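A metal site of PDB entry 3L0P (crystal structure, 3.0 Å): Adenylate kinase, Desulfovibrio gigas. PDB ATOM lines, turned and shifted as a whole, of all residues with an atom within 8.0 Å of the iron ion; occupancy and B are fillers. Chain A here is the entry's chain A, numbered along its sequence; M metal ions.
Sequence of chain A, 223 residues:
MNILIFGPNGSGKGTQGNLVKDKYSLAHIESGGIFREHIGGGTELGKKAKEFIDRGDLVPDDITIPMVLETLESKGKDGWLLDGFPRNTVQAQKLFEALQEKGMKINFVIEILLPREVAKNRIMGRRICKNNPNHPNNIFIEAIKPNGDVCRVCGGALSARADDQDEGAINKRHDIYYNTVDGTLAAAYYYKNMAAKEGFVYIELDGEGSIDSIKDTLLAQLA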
ATOM      1  N   ILE A 128     -28.082  27.722 -12.357  1.00  0.00           N
ATOM      2  CA  ILE A 128     -27.363  27.040 -11.240  1.00  0.00           C
ATOM      3  C   ILE A 128     -25.926  26.567 -11.598  1.00  0.00           C
ATOM      4  O   ILE A 128     -25.756  25.674 -12.447  1.00  0.00           O
ATOM      5  CB  ILE A 128     -28.191  25.801 -10.649  1.00  0.00           C
ATOM      6  CG1 ILE A 128     -29.680  26.105 -10.521  1.00  0.00           C
ATOM      7  CG2 ILE A 128     -27.596  25.251  -9.329  1.00  0.00           C
ATOM      8  CD1 ILE A 128     -29.985  27.406  -9.790  1.00  0.00           C
ATOM      9  N   CYS A 129     -24.924  27.142 -10.923  1.00  0.00           N
ATOM     10  CA  CYS A 129     -23.535  26.654 -11.009  1.00  0.00           C
ATOM     11  C   CYS A 129     -23.417  25.209 -10.556  1.00  0.00           C
ATOM     12  O   CYS A 129     -23.867  24.861  -9.483  1.00  0.00           O
ATOM     13  CB  CYS A 129     -22.610  27.560 -10.178  1.00  0.00           C
ATOM     14  SG  CYS A 129     -20.874  26.947  -9.840  1.00  0.00           S
ATOM     15  N   LYS A 130     -22.820  24.390 -11.405  1.00  0.00           N
ATOM     16  CA  LYS A 130     -22.642  22.956 -11.159  1.00  0.00           C
ATOM     17  C   LYS A 130     -21.614  22.627 -10.050  1.00  0.00           C
ATOM     18  O   LYS A 130     -21.655  21.534  -9.472  1.00  0.00           O
ATOM     19  CB  LYS A 130     -22.227  22.234 -12.436  1.00  0.00           C
ATOM     20  CG  LYS A 130     -22.189  20.715 -12.311  1.00  0.00           C
ATOM     21  CD  LYS A 130     -21.773  20.034 -13.604  1.00  0.00           C
ATOM     22  CE  LYS A 130     -20.272  19.899 -13.742  1.00  0.00           C
ATOM     23  NZ  LYS A 130     -20.048  18.905 -14.793  1.00  0.00           N
ATOM     24  N   ASN A 131     -20.702  23.547  -9.768  1.00  0.00           N
ATOM     25  CA  ASN A 131     -19.726  23.364  -8.691  1.00  0.00           C
ATOM     26  C   ASN A 131     -20.366  23.544  -7.325  1.00  0.00           C
ATOM     27  O   ASN A 131     -20.162  22.733  -6.408  1.00  0.00           O
ATOM     28  CB  ASN A 131     -18.573  24.363  -8.810  1.00  0.00           C
ATOM     29  CG  ASN A 131     -17.739  24.135 -10.024  1.00  0.00           C
ATOM     30  OD1 ASN A 131     -17.470  22.994 -10.434  1.00  0.00           O
ATOM     31  ND2 ASN A 131     -17.284  25.230 -10.609  1.00  0.00           N
ATOM     32  N   ASN A 132     -21.118  24.626  -7.180  1.00  0.00           N
ATOM     33  CA  ASN A 132     -21.675  24.951  -5.916  1.00  0.00           C
ATOM     34  C   ASN A 132     -22.957  25.668  -6.189  1.00  0.00           C
ATOM     35  O   ASN A 132     -22.943  26.809  -6.647  1.00  0.00           O
ATOM     36  CB  ASN A 132     -20.716  25.848  -5.141  1.00  0.00           C
ATOM     37  CG  ASN A 132     -21.142  26.071  -3.693  1.00  0.00           C
ATOM     38  OD1 ASN A 132     -20.337  25.847  -2.787  1.00  0.00           O
ATOM     39  ND2 ASN A 132     -22.361  26.540  -3.478  1.00  0.00           N
ATOM     40  N   PRO A 133     -24.075  24.995  -5.870  1.00  0.00           N
ATOM     41  CA  PRO A 133     -25.409  25.463  -6.213  1.00  0.00           C
ATOM     42  C   PRO A 133     -25.764  26.782  -5.511  1.00  0.00           C
ATOM     43  O   PRO A 133     -26.550  27.533  -6.068  1.00  0.00           O
ATOM     44  CB  PRO A 133     -26.304  24.329  -5.744  1.00  0.00           C
ATOM     45  CG  PRO A 133     -25.554  23.694  -4.618  1.00  0.00           C
ATOM     46  CD  PRO A 133     -24.123  23.814  -4.987  1.00  0.00           C
ATOM     47  N   ASN A 134     -25.156  27.062  -4.346  1.00  0.00           N
ATOM     48  CA  ASN A 134     -25.387  28.330  -3.632  1.00  0.00           C
ATOM     49  C   ASN A 134     -24.918  29.578  -4.340  1.00  0.00           C
ATOM     50  O   ASN A 134     -25.245  30.673  -3.893  1.00  0.00           O
ATOM     51  CB  ASN A 134     -24.664  28.389  -2.281  1.00  0.00           C
ATOM     52  CG  ASN A 134     -25.033  27.266  -1.365  1.00  0.00           C
ATOM     53  OD1 ASN A 134     -26.128  26.663  -1.483  1.00  0.00           O
ATOM     54  ND2 ASN A 134     -24.128  26.975  -0.417  1.00  0.00           N
ATOM     55  N   HIS A 135     -24.107  29.432  -5.377  1.00  0.00           N
ATOM     56  CA  HIS A 135     -23.520  30.596  -6.047  1.00  0.00           C
ATOM     57  C   HIS A 135     -24.600  31.298  -6.884  1.00  0.00           C
ATOM     58  O   HIS A 135     -24.954  30.793  -7.948  1.00  0.00           O
ATOM     59  CB  HIS A 135     -22.367  30.172  -6.953  1.00  0.00           C
ATOM     60  CG  HIS A 135     -21.135  29.734  -6.231  1.00  0.00           C
ATOM     61  ND1 HIS A 135     -20.149  28.991  -6.850  1.00  0.00           N
ATOM     62  CD2 HIS A 135     -20.710  29.932  -4.970  1.00  0.00           C
ATOM     63  CE1 HIS A 135     -19.170  28.761  -5.996  1.00  0.00           C
ATOM     64  NE2 HIS A 135     -19.492  29.326  -4.843  1.00  0.00           N
ATOM     65  N   PRO A 136     -25.068  32.484  -6.422  1.00  0.00           N
ATOM     66  CA  PRO A 136     -26.241  33.116  -7.029  1.00  0.00           C
ATOM     67  C   PRO A 136     -25.959  33.770  -8.392  1.00  0.00           C
ATOM     68  O   PRO A 136     -25.244  34.772  -8.480  1.00  0.00           O
ATOM     69  CB  PRO A 136     -26.651  34.170  -5.984  1.00  0.00           C
ATOM     70  CG  PRO A 136     -25.747  33.967  -4.828  1.00  0.00           C
ATOM     71  CD  PRO A 136     -24.532  33.364  -5.374  1.00  0.00           C
ATOM     72  N   ASN A 137     -26.524  33.179  -9.440  1.00  0.00           N
ATOM     73  CA  ASN A 137     -26.431  33.678 -10.815  1.00  0.00           C
ATOM     74  C   ASN A 137     -27.828  33.922 -11.368  1.00  0.00           C
ATOM     75  O   ASN A 137     -28.721  33.061 -11.239  1.00  0.00           O
ATOM     76  CB  ASN A 137     -25.692  32.671 -11.728  1.00  0.00           C
ATOM     77  CG  ASN A 137     -24.257  32.390 -11.299  1.00  0.00           C
ATOM     78  OD1 ASN A 137     -23.912  31.276 -10.898  1.00  0.00           O
ATOM     79  ND2 ASN A 137     -23.420  33.398 -11.377  1.00  0.00           N
ATOM     80  N   VAL A 150     -21.161  30.844 -17.897  1.00  0.00           N
ATOM     81  CA  VAL A 150     -20.561  30.216 -16.652  1.00  0.00           C
ATOM     82  C   VAL A 150     -20.551  31.099 -15.363  1.00  0.00           C
ATOM     83  O   VAL A 150     -20.737  32.329 -15.411  1.00  0.00           O
ATOM     84  CB  VAL A 150     -19.121  29.555 -16.853  1.00  0.00           C
ATOM     85  CG1 VAL A 150     -18.986  28.793 -18.182  1.00  0.00           C
ATOM     86  CG2 VAL A 150     -18.033  30.568 -16.726  1.00  0.00           C
ATOM     87  N   CYS A 151     -20.321  30.447 -14.221  1.00  0.00           N
ATOM     88  CA  CYS A 151     -20.607  31.048 -12.917  1.00  0.00           C
ATOM     89  C   CYS A 151     -19.879  32.352 -12.602  1.00  0.00           C
ATOM     90  O   CYS A 151     -18.670  32.415 -12.623  1.00  0.00           O
ATOM     91  CB  CYS A 151     -20.360  30.025 -11.805  1.00  0.00           C
ATOM     92  SG  CYS A 151     -20.641  30.594 -10.091  1.00  0.00           S
ATOM     93  N   ARG A 152     -20.670  33.385 -12.330  1.00  0.00           N
ATOM     94  CA  ARG A 152     -20.205  34.651 -11.765  1.00  0.00           C
ATOM     95  C   ARG A 152     -19.151  34.467 -10.677  1.00  0.00           C
ATOM     96  O   ARG A 152     -18.229  35.234 -10.581  1.00  0.00           O
ATOM     97  CB  ARG A 152     -21.398  35.399 -11.158  1.00  0.00           C
ATOM     98  CG  ARG A 152     -21.123  36.797 -10.682  1.00  0.00           C
ATOM     99  CD  ARG A 152     -22.383  37.440 -10.160  1.00  0.00           C
ATOM    100  NE  ARG A 152     -22.454  37.459  -8.707  1.00  0.00           N
ATOM    101  CZ  ARG A 152     -22.617  36.375  -7.960  1.00  0.00           C
ATOM    102  NH1 ARG A 152     -22.690  35.200  -8.543  1.00  0.00           N
ATOM    103  NH2 ARG A 152     -22.708  36.466  -6.631  1.00  0.00           N
ATOM    104  N   VAL A 153     -19.307  33.439  -9.838  1.00  0.00           N
ATOM    105  CA  VAL A 153     -18.418  33.244  -8.700  1.00  0.00           C
ATOM    106  C   VAL A 153     -17.158  32.467  -9.030  1.00  0.00           C
ATOM    107  O   VAL A 153     -16.052  32.950  -8.792  1.00  0.00           O
ATOM    108  CB  VAL A 153     -19.114  32.554  -7.470  1.00  0.00           C
ATOM    109  CG1 VAL A 153     -18.069  32.229  -6.374  1.00  0.00           C
ATOM    110  CG2 VAL A 153     -20.316  33.391  -6.930  1.00  0.00           C
ATOM    111  N   CYS A 154     -17.302  31.262  -9.558  1.00  0.00           N
ATOM    112  CA  CYS A 154     -16.129  30.425  -9.707  1.00  0.00           C
ATOM    113  C   CYS A 154     -15.883  29.977 -11.137  1.00  0.00           C
ATOM    114  O   CYS A 154     -14.924  29.249 -11.433  1.00  0.00           O
ATOM    115  CB  CYS A 154     -16.250  29.229  -8.783  1.00  0.00           C
ATOM    116  SG  CYS A 154     -17.444  28.026  -9.384  1.00  0.00           S
ATOM    117  N   GLY A 155     -16.755  30.405 -12.020  1.00  0.00           N
ATOM    118  CA  GLY A 155     -16.642  30.014 -13.398  1.00  0.00           C
ATOM    119  C   GLY A 155     -16.886  28.544 -13.657  1.00  0.00           C
ATOM    120  O   GLY A 155     -16.247  27.975 -14.530  1.00  0.00           O
ATOM    121  N   GLY A 156     -17.786  27.914 -12.899  1.00  0.00           N
ATOM    122  CA  GLY A 156     -18.214  26.542 -13.210  1.00  0.00           C
ATOM    123  C   GLY A 156     -19.325  26.605 -14.222  1.00  0.00           C
ATOM    124  O   GLY A 156     -19.954  27.666 -14.396  1.00  0.00           O
ATOM    125  N   ALA A 157     -19.576  25.493 -14.918  1.00  0.00           N
ATOM    126  CA  ALA A 157     -20.758  25.389 -15.809  1.00  0.00           C
ATOM    127  C   ALA A 157     -22.035  25.598 -15.011  1.00  0.00           C
ATOM    128  O   ALA A 157     -22.198  25.043 -13.910  1.00  0.00           O
ATOM    129  CB  ALA A 157     -20.819  24.048 -16.563  1.00  0.00           C
ATOM    130  N   LEU A 158     -22.921  26.418 -15.582  1.00  0.00           N
ATOM    131  CA  LEU A 158     -24.235  26.694 -14.990  1.00  0.00           C
ATOM    132  C   LEU A 158     -25.369  26.315 -15.925  1.00  0.00           C
ATOM    133  O   LEU A 158     -25.301  26.582 -17.111  1.00  0.00           O
ATOM    134  CB  LEU A 158     -24.328  28.151 -14.458  1.00  0.00           C
ATOM    135  CG  LEU A 158     -24.513  29.457 -15.234  1.00  0.00           C
ATOM    136  CD1 LEU A 158     -23.769  30.611 -14.552  1.00  0.00           C
ATOM    137  CD2 LEU A 158     -24.164  29.393 -16.699  1.00  0.00           C
HETATM  138 FE    FE M   1     -20.105  28.728  -8.965  1.00  0.00          FE
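OD1 of Asn 137 sits close to SG of Cys 151 (3.4 Å). The side-chain sulfur (SG) of Cys 129 lies close to the backbone NH (N) of Asn 132 (3.5 Å). The backbone NH (N) of Gly 156 lies close to the side-chain sulfur (SG) of Cys 154, 3.5 Å away. OD1 of Asn 137 lies close to O of His 135, 3.2 Å away. The side-chain sulfur of Cys 129 lies close to the backbone NH of Asn 131, 3.4 Å away. The side-chain sulfur (SG) of Cys 154 lies close to the side-chain amide nitrogen (ND2) of Asn 131 (3.1 Å). The side-chain sulfur (SG) of Cys 151 sits close to the backbone NH (N) of Val 153 (3.2 Å). N of Cys 151 lies within hydrogen-bond range of O of Gly 156.
The nearest printed residue that does not touch the iron ion is Asn 132 (4.1 Å).
The iron ion is bound by SG of Cys 129 (2.1 Å), ND1 of His 135 (2.1 Å), SG of Cys 151 (2.2 Å) and SG of Cys 154 (2.8 Å).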
